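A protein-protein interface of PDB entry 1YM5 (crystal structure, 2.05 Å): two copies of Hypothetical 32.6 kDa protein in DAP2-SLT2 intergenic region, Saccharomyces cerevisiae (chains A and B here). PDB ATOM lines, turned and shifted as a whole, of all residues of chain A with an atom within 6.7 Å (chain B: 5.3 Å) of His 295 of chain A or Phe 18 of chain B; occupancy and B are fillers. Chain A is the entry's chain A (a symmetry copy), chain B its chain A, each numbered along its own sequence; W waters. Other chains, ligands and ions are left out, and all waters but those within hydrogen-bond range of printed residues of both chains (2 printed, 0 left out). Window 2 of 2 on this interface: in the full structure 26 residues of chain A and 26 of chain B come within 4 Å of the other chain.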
ATOM      1  N   LEU A   3       0.840   0.440  18.398  1.00  0.00           N
ATOM      2  CA  LEU A   3       1.309  -0.429  17.294  1.00  0.00           C
ATOM      3  C   LEU A   3       0.779   0.050  15.918  1.00  0.00           C
ATOM      4  O   LEU A   3      -0.409   0.164  15.690  1.00  0.00           O
ATOM      5  CB  LEU A   3       0.971  -1.889  17.504  1.00  0.00           C
ATOM      6  CG  LEU A   3       1.697  -2.777  16.482  1.00  0.00           C
ATOM      7  CD1 LEU A   3       3.200  -2.821  16.693  1.00  0.00           C
ATOM      8  CD2 LEU A   3       1.144  -4.175  16.476  1.00  0.00           C
ATOM      9  N   PHE A  28       0.105  -7.414   7.774  1.00  0.00           N
ATOM     10  CA  PHE A  28       0.281  -8.208   9.023  1.00  0.00           C
ATOM     11  C   PHE A  28       1.314  -9.343   8.853  1.00  0.00           C
ATOM     12  O   PHE A  28       1.281 -10.378   9.563  1.00  0.00           O
ATOM     13  CB  PHE A  28      -1.070  -8.803   9.453  1.00  0.00           C
ATOM     14  CG  PHE A  28      -1.961  -7.870  10.270  1.00  0.00           C
ATOM     15  CD1 PHE A  28      -1.427  -6.969  11.160  1.00  0.00           C
ATOM     16  CD2 PHE A  28      -3.329  -7.982  10.195  1.00  0.00           C
ATOM     17  CE1 PHE A  28      -2.220  -6.181  11.948  1.00  0.00           C
ATOM     18  CE2 PHE A  28      -4.152  -7.173  10.939  1.00  0.00           C
ATOM     19  CZ  PHE A  28      -3.596  -6.271  11.833  1.00  0.00           C
ATOM     20  N   ILE A  31       3.336 -10.096  12.041  1.00  0.00           N
ATOM     21  CA  ILE A  31       2.637 -10.477  13.270  1.00  0.00           C
ATOM     22  C   ILE A  31       1.894 -11.839  13.114  1.00  0.00           C
ATOM     23  O   ILE A  31       1.542 -12.268  12.015  1.00  0.00           O
ATOM     24  CB  ILE A  31       1.663  -9.372  13.749  1.00  0.00           C
ATOM     25  CG1 ILE A  31       0.485  -9.240  12.817  1.00  0.00           C
ATOM     26  CG2 ILE A  31       2.366  -7.967  13.927  1.00  0.00           C
ATOM     27  CD1 ILE A  31      -0.852  -9.689  13.439  1.00  0.00           C
ATOM     28  N   GLU A  35      -2.915 -14.420  16.776  1.00  0.00           N
ATOM     29  CA  GLU A  35      -3.108 -13.374  17.756  1.00  0.00           C
ATOM     30  C   GLU A  35      -4.006 -12.233  17.241  1.00  0.00           C
ATOM     31  O   GLU A  35      -3.961 -11.130  17.791  1.00  0.00           O
ATOM     32  CB  GLU A  35      -1.727 -12.817  18.174  1.00  0.00           C
ATOM     33  CG  GLU A  35      -0.808 -13.844  18.905  1.00  0.00           C
ATOM     34  CD  GLU A  35       0.704 -13.471  18.879  1.00  0.00           C
ATOM     35  OE1 GLU A  35       1.033 -12.361  18.379  1.00  0.00           O
ATOM     36  OE2 GLU A  35       1.558 -14.298  19.349  1.00  0.00           O
ATOM     37  N   VAL A  36      -4.805 -12.472  16.192  1.00  0.00           N
ATOM     38  CA  VAL A  36      -5.651 -11.414  15.613  1.00  0.00           C
ATOM     39  C   VAL A  36      -7.013 -12.014  15.365  1.00  0.00           C
ATOM     40  O   VAL A  36      -7.153 -12.939  14.577  1.00  0.00           O
ATOM     41  CB  VAL A  36      -5.102 -10.867  14.268  1.00  0.00           C
ATOM     42  CG1 VAL A  36      -5.947  -9.707  13.761  1.00  0.00           C
ATOM     43  CG2 VAL A  36      -3.662 -10.412  14.416  1.00  0.00           C
ATOM     44  N   GLU A  40     -11.798  -8.161  15.096  1.00  0.00           N
ATOM     45  CA  GLU A  40     -10.797  -7.118  14.866  1.00  0.00           C
ATOM     46  C   GLU A  40     -10.655  -6.832  13.361  1.00  0.00           C
ATOM     47  O   GLU A  40     -10.793  -5.678  12.912  1.00  0.00           O
ATOM     48  CB  GLU A  40      -9.481  -7.670  15.414  1.00  0.00           C
ATOM     49  CG  GLU A  40      -8.389  -6.749  15.776  1.00  0.00           C
ATOM     50  CD  GLU A  40      -7.477  -7.445  16.801  1.00  0.00           C
ATOM     51  OE1 GLU A  40      -6.290  -7.681  16.451  1.00  0.00           O
ATOM     52  OE2 GLU A  40      -7.971  -7.783  17.944  1.00  0.00           O
ATOM     53  N   LEU A  41     -10.415  -7.898  12.588  1.00  0.00           N
ATOM     54  CA  LEU A  41     -10.304  -7.790  11.144  1.00  0.00           C
ATOM     55  C   LEU A  41     -11.586  -7.209  10.526  1.00  0.00           C
ATOM     56  O   LEU A  41     -11.543  -6.230   9.765  1.00  0.00           O
ATOM     57  CB  LEU A  41      -9.922  -9.144  10.520  1.00  0.00           C
ATOM     58  CG  LEU A  41      -8.580  -9.787  10.942  1.00  0.00           C
ATOM     59  CD1 LEU A  41      -8.323 -11.064  10.176  1.00  0.00           C
ATOM     60  CD2 LEU A  41      -7.402  -8.876  10.829  1.00  0.00           C
ATOM     61  N   ALA A  43     -13.918  -5.386  11.955  1.00  0.00           N
ATOM     62  CA  ALA A  43     -14.111  -4.032  12.419  1.00  0.00           C
ATOM     63  C   ALA A  43     -13.308  -3.063  11.571  1.00  0.00           C
ATOM     64  O   ALA A  43     -13.770  -1.989  11.258  1.00  0.00           O
ATOM     65  CB  ALA A  43     -13.658  -3.926  13.894  1.00  0.00           C
ATOM     66  N   ILE A  44     -12.072  -3.439  11.225  1.00  0.00           N
ATOM     67  CA  ILE A  44     -11.238  -2.605  10.375  1.00  0.00           C
ATOM     68  C   ILE A  44     -11.852  -2.441   8.999  1.00  0.00           C
ATOM     69  O   ILE A  44     -11.855  -1.347   8.438  1.00  0.00           O
ATOM     70  CB  ILE A  44      -9.798  -3.192  10.282  1.00  0.00           C
ATOM     71  CG1 ILE A  44      -9.127  -3.147  11.659  1.00  0.00           C
ATOM     72  CG2 ILE A  44      -8.931  -2.403   9.306  1.00  0.00           C
ATOM     73  CD1 ILE A  44      -7.730  -3.749  11.641  1.00  0.00           C
ATOM     74  N   ALA A  45     -12.393  -3.528   8.460  1.00  0.00           N
ATOM     75  CA  ALA A  45     -13.010  -3.519   7.131  1.00  0.00           C
ATOM     76  C   ALA A  45     -14.300  -2.694   7.111  1.00  0.00           C
ATOM     77  O   ALA A  45     -14.628  -2.032   6.127  1.00  0.00           O
ATOM     78  CB  ALA A  45     -13.295  -4.962   6.683  1.00  0.00           C
ATOM     79  N   ASN A  46     -15.031  -2.764   8.222  1.00  0.00           N
ATOM     80  CA  ASN A  46     -16.257  -2.016   8.374  1.00  0.00           C
ATOM     81  C   ASN A  46     -15.949  -0.543   8.477  1.00  0.00           C
ATOM     82  O   ASN A  46     -16.612   0.266   7.845  1.00  0.00           O
ATOM     83  CB  ASN A  46     -16.984  -2.479   9.614  1.00  0.00           C
ATOM     84  CG  ASN A  46     -18.328  -1.859   9.733  1.00  0.00           C
ATOM     85  OD1 ASN A  46     -18.465  -0.890  10.429  1.00  0.00           O
ATOM     86  ND2 ASN A  46     -19.296  -2.337   8.973  1.00  0.00           N
ATOM     87  N   TRP A  47     -14.895  -0.210   9.231  1.00  0.00           N
ATOM     88  CA  TRP A  47     -14.467   1.186   9.390  1.00  0.00           C
ATOM     89  C   TRP A  47     -13.911   1.855   8.128  1.00  0.00           C
ATOM     90  O   TRP A  47     -14.128   3.054   7.883  1.00  0.00           O
ATOM     91  CB  TRP A  47     -13.423   1.232  10.517  1.00  0.00           C
ATOM     92  CG  TRP A  47     -12.957   2.616  10.839  1.00  0.00           C
ATOM     93  CD1 TRP A  47     -13.575   3.509  11.661  1.00  0.00           C
ATOM     94  CD2 TRP A  47     -11.738   3.250  10.408  1.00  0.00           C
ATOM     95  NE1 TRP A  47     -12.837   4.655  11.757  1.00  0.00           N
ATOM     96  CE2 TRP A  47     -11.710   4.531  10.990  1.00  0.00           C
ATOM     97  CE3 TRP A  47     -10.682   2.868   9.562  1.00  0.00           C
ATOM     98  CZ2 TRP A  47     -10.661   5.427  10.770  1.00  0.00           C
ATOM     99  CZ3 TRP A  47      -9.642   3.762   9.356  1.00  0.00           C
ATOM    100  CH2 TRP A  47      -9.636   5.010   9.962  1.00  0.00           C
ATOM    101  N   THR A  48     -13.122   1.137   7.331  1.00  0.00           N
ATOM    102  CA  THR A  48     -12.651   1.750   6.059  1.00  0.00           C
ATOM    103  C   THR A  48     -13.823   1.969   5.098  1.00  0.00           C
ATOM    104  O   THR A  48     -13.782   2.889   4.259  1.00  0.00           O
ATOM    105  CB  THR A  48     -11.645   0.876   5.322  1.00  0.00           C
ATOM    106  OG1 THR A  48     -12.313  -0.280   4.756  1.00  0.00           O
ATOM    107  CG2 THR A  48     -10.564   0.440   6.244  1.00  0.00           C
ATOM    108  N   ILE A 292      -0.946   2.096   9.655  1.00  0.00           N
ATOM    109  CA  ILE A 292      -2.250   2.083  10.290  1.00  0.00           C
ATOM    110  C   ILE A 292      -2.102   1.569  11.697  1.00  0.00           C
ATOM    111  O   ILE A 292      -1.402   0.618  11.921  1.00  0.00           O
ATOM    112  CB  ILE A 292      -3.236   1.171   9.472  1.00  0.00           C
ATOM    113  CG1 ILE A 292      -4.674   1.281   9.989  1.00  0.00           C
ATOM    114  CG2 ILE A 292      -2.791  -0.328   9.441  1.00  0.00           C
ATOM    115  CD1 ILE A 292      -5.681   0.782   9.004  1.00  0.00           C
ATOM    116  N   LYS A 293      -2.767   2.210  12.653  1.00  0.00           N
ATOM    117  CA  LYS A 293      -2.793   1.760  14.055  1.00  0.00           C
ATOM    118  C   LYS A 293      -3.650   0.547  14.258  1.00  0.00           C
ATOM    119  O   LYS A 293      -4.831   0.535  13.847  1.00  0.00           O
ATOM    120  CB  LYS A 293      -3.428   2.818  14.929  1.00  0.00           C
ATOM    121  CG  LYS A 293      -2.583   3.942  15.264  1.00  0.00           C
ATOM    122  CD  LYS A 293      -3.315   4.846  16.199  1.00  0.00           C
ATOM    123  CE  LYS A 293      -2.500   6.062  16.532  1.00  0.00           C
ATOM    124  NZ  LYS A 293      -3.397   7.121  16.967  1.00  0.00           N
ATOM    125  N   VAL A 294      -3.096  -0.452  14.921  1.00  0.00           N
ATOM    126  CA  VAL A 294      -3.777  -1.697  15.161  1.00  0.00           C
ATOM    127  C   VAL A 294      -3.550  -2.145  16.609  1.00  0.00           C
ATOM    128  O   VAL A 294      -2.683  -1.611  17.309  1.00  0.00           O
ATOM    129  CB  VAL A 294      -3.275  -2.812  14.200  1.00  0.00           C
ATOM    130  CG1 VAL A 294      -3.404  -2.367  12.711  1.00  0.00           C
ATOM    131  CG2 VAL A 294      -1.869  -3.251  14.534  1.00  0.00           C
ATOM    132  N   HIS A 295      -4.287  -3.182  17.012  1.00  0.00           N
ATOM    133  CA  HIS A 295      -4.386  -3.606  18.393  1.00  0.00           C
ATOM    134  C   HIS A 295      -3.437  -4.787  18.536  1.00  0.00           C
ATOM    135  O   HIS A 295      -3.607  -5.813  17.831  1.00  0.00           O
ATOM    136  CB  HIS A 295      -5.841  -4.029  18.769  1.00  0.00           C
ATOM    137  CG  HIS A 295      -6.909  -3.641  17.760  1.00  0.00           C
ATOM    138  ND1 HIS A 295      -6.856  -3.999  16.413  1.00  0.00           N
ATOM    139  CD2 HIS A 295      -8.098  -2.997  17.925  1.00  0.00           C
ATOM    140  CE1 HIS A 295      -7.949  -3.564  15.797  1.00  0.00           C
ATOM    141  NE2 HIS A 295      -8.723  -2.968  16.690  1.00  0.00           N
ATOM    142  N   ASP B  11     -10.067   9.219  13.187  1.00  0.00           N
ATOM    143  CA  ASP B  11     -11.290   8.666  13.730  1.00  0.00           C
ATOM    144  C   ASP B  11     -11.863   9.675  14.720  1.00  0.00           C
ATOM    145  O   ASP B  11     -11.197  10.045  15.711  1.00  0.00           O
ATOM    146  CB  ASP B  11     -10.962   7.325  14.418  1.00  0.00           C
ATOM    147  CG  ASP B  11     -12.084   6.316  14.346  1.00  0.00           C
ATOM    148  OD1 ASP B  11     -11.961   5.270  15.049  1.00  0.00           O
ATOM    149  OD2 ASP B  11     -13.098   6.573  13.638  1.00  0.00           O
ATOM    150  N   LYS B  16      -9.958   5.594  20.817  1.00  0.00           N
ATOM    151  CA  LYS B  16      -9.659   4.222  20.401  1.00  0.00           C
ATOM    152  C   LYS B  16      -9.925   4.005  18.918  1.00  0.00           C
ATOM    153  O   LYS B  16     -11.043   4.209  18.451  1.00  0.00           O
ATOM    154  CB  LYS B  16     -10.493   3.222  21.216  1.00  0.00           C
ATOM    155  CG  LYS B  16     -10.299   3.410  22.745  1.00  0.00           C
ATOM    156  CD  LYS B  16     -11.084   2.356  23.583  1.00  0.00           C
ATOM    157  CE  LYS B  16     -10.815   2.585  25.102  1.00  0.00           C
ATOM    158  NZ  LYS B  16     -11.363   1.403  25.889  1.00  0.00           N
ATOM    159  N   PRO B  17      -8.902   3.587  18.171  1.00  0.00           N
ATOM    160  CA  PRO B  17      -9.041   3.356  16.734  1.00  0.00           C
ATOM    161  C   PRO B  17     -10.192   2.443  16.279  1.00  0.00           C
ATOM    162  O   PRO B  17     -10.500   1.446  16.939  1.00  0.00           O
ATOM    163  CB  PRO B  17      -7.701   2.739  16.366  1.00  0.00           C
ATOM    164  CG  PRO B  17      -6.762   3.340  17.318  1.00  0.00           C
ATOM    165  CD  PRO B  17      -7.509   3.363  18.617  1.00  0.00           C
ATOM    166  N   PHE B  18     -10.800   2.781  15.140  1.00  0.00           N
ATOM    167  CA  PHE B  18     -11.895   2.009  14.569  1.00  0.00           C
ATOM    168  C   PHE B  18     -13.230   2.098  15.363  1.00  0.00           C
ATOM    169  O   PHE B  18     -14.233   1.517  14.955  1.00  0.00           O
ATOM    170  CB  PHE B  18     -11.521   0.546  14.266  1.00  0.00           C
ATOM    171  CG  PHE B  18     -10.174   0.376  13.632  1.00  0.00           C
ATOM    172  CD1 PHE B  18      -9.962   0.778  12.327  1.00  0.00           C
ATOM    173  CD2 PHE B  18      -9.112  -0.125  14.360  1.00  0.00           C
ATOM    174  CE1 PHE B  18      -8.722   0.690  11.764  1.00  0.00           C
ATOM    175  CE2 PHE B  18      -7.868  -0.283  13.776  1.00  0.00           C
ATOM    176  CZ  PHE B  18      -7.657   0.175  12.487  1.00  0.00           C
ATOM    177  N   MET B  19     -13.268   2.884  16.438  1.00  0.00           N
ATOM    178  CA  MET B  19     -14.509   3.033  17.222  1.00  0.00           C
ATOM    179  C   MET B  19     -15.342   4.286  16.880  1.00  0.00           C
ATOM    180  O   MET B  19     -16.486   4.476  17.363  1.00  0.00           O
ATOM    181  CB  MET B  19     -14.187   2.977  18.734  1.00  0.00           C
ATOM    182  CG  MET B  19     -13.573   1.643  19.132  1.00  0.00           C
ATOM    183  SD  MET B  19     -14.800   0.305  18.877  1.00  0.00           S
ATOM    184  CE  MET B  19     -13.661  -0.952  18.385  1.00  0.00           C
ATOM    185  N   GLY B  20     -14.786   5.153  16.068  1.00  0.00           N
ATOM    186  CA  GLY B  20     -15.426   6.458  15.807  1.00  0.00           C
ATOM    187  C   GLY B  20     -15.864   6.519  14.378  1.00  0.00           C
ATOM    188  O   GLY B  20     -16.040   5.505  13.709  1.00  0.00           O
ATOM    189  N   LYS B 259     -21.120  -2.064  16.489  1.00  0.00           N
ATOM    190  CA  LYS B 259     -19.797  -2.380  17.007  1.00  0.00           C
ATOM    191  C   LYS B 259     -18.848  -1.207  16.948  1.00  0.00           C
ATOM    192  O   LYS B 259     -17.645  -1.402  16.863  1.00  0.00           O
ATOM    193  CB  LYS B 259     -19.225  -3.628  16.270  1.00  0.00           C
ATOM    194  CG  LYS B 259     -20.208  -4.819  16.282  1.00  0.00           C
ATOM    195  CD  LYS B 259     -19.490  -6.152  16.195  1.00  0.00           C
ATOM    196  CE  LYS B 259     -20.466  -7.269  15.800  1.00  0.00           C
ATOM    197  NZ  LYS B 259     -20.902  -7.042  14.376  1.00  0.00           N
ATOM    198  N   ARG B 260     -19.352   0.021  17.058  1.00  0.00           N
ATOM    199  CA  ARG B 260     -18.500   1.177  17.376  1.00  0.00           C
ATOM    200  C   ARG B 260     -18.785   1.729  18.799  1.00  0.00           C
ATOM    201  O   ARG B 260     -19.575   1.202  19.547  1.00  0.00           O
ATOM    202  CB  ARG B 260     -18.662   2.315  16.344  1.00  0.00           C
ATOM    203  CG  ARG B 260     -18.690   1.918  14.888  1.00  0.00           C
ATOM    204  CD  ARG B 260     -17.413   2.215  14.212  1.00  0.00           C
ATOM    205  NE  ARG B 260     -17.482   1.820  12.822  1.00  0.00           N
ATOM    206  CZ  ARG B 260     -17.497   2.618  11.778  1.00  0.00           C
ATOM    207  NH1 ARG B 260     -17.441   3.914  11.890  1.00  0.00           N
ATOM    208  NH2 ARG B 260     -17.597   2.082  10.579  1.00  0.00           N
ATOM    209  N   VAL B 287      -5.647   7.329  12.703  1.00  0.00           N
ATOM    210  CA  VAL B 287      -5.583   5.891  12.592  1.00  0.00           C
ATOM    211  C   VAL B 287      -4.659   5.459  11.435  1.00  0.00           C
ATOM    212  O   VAL B 287      -3.904   4.499  11.570  1.00  0.00           O
ATOM    213  CB  VAL B 287      -7.006   5.314  12.343  1.00  0.00           C
ATOM    214  CG1 VAL B 287      -7.025   3.795  12.101  1.00  0.00           C
ATOM    215  CG2 VAL B 287      -7.904   5.642  13.555  1.00  0.00           C
HETATM  216  O   HOH W   1     -16.745   4.106   8.306  1.00  0.00           O
HETATM  217  O   HOH W   2     -15.757  -0.801  12.828  1.00  0.00           O
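No position is printed for both chains.
The guanidinium group (NH2) of Arg 260 of chain B lies within hydrogen-bond range of the side-chain amide oxygen (OD1) of Asn 46 of chain A (3.1 Å).
OD2 of Asp 11 of chain B lies within hydrogen-bond range of NE1 of Trp 47 of chain A (2.7 Å).
N of Lys 293 of chain A sits at hydrogen-bond distance from O of Val 287 of chain B, at 2.8 Å.
Of the 9 printed residues of chain B, 6 touch a printed residue of chain A.
Hydrophobic or aromatic side chains of chain B that line the printed part of chain A: Pro 17, Phe 18 and Val 287.
Printed residues of chain A that touch a printed residue of chain B: Ile 44, Asn 46, Trp 47, Ile 292, Lys 293 and His 295.
Hydrophobic or aromatic side chains of chain A that line the printed part of chain B: Ile 44, Trp 47, Ile 292 and His 295.
Among the printed residues, 12 pairs touch across the chains.
N of Gly 20 of chain B is in hydrogen-bond range of OD1 of Asp 11 of chain B (3.0 Å).
OD1 of Asp 11 of chain B lies within hydrogen-bond range of N of Phe 18 of chain B, 2.7 Å away.
The side-chain carboxylate (OD1) of Asp 11 of chain B lies within hydrogen-bond range of the backbone NH (N) of Met 19 of chain B (3.1 Å).
O of Gly 20 of chain B is in hydrogen-bond range of NH1 of Arg 260 of chain B (2.8 Å).
Water W2 lies within hydrogen-bond range of O of Ala 43 of chain A (2.8 Å), NE of Arg 260 of chain B (3.1 Å) and O of Phe 18 of chain B (3.5 Å).
Water W1 bridges O of Trp 47 of chain A (2.9 Å) and NH2 of Arg 260 of chain B (3.2 Å).
Of the printed residues of chain B, Trp 47 of chain A touches Asp 11, Phe 18, Gly 20, Arg 260 and Val 287.
Thr 48 of chain A touches none of the printed residues of chain B.
His 295 of chain A touches just one residue of chain B: Phe 18 (3.7 Å).
Of the printed residues of chain A, Phe 18 of chain B touches Ile 44, Trp 47, Lys 293 and His 295.
Printed residues of chain A within 4 Å of Gly 20 of chain B: Trp 47.
Printed residues of chain A within 4 Å of Arg 260 of chain B: Asn 46 and Trp 47.
Among the printed residues, merely in contact across the chains: Ile 44 of chain A with Phe 18 of chain B, Trp 47 of chain A with Phe 18 of chain B, Trp 47 of chain A with Gly 20 of chain B, Trp 47 of chain A with Arg 260 of chain B, Trp 47 of chain A with Val 287 of chain B, Ile 292 of chain A with Val 287 of chain B, Lys 293 of chain A with Pro 17 of chain B, Lys 293 of chain A with Phe 18 of chain B and His 295 of chain A with Phe 18 of chain B.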
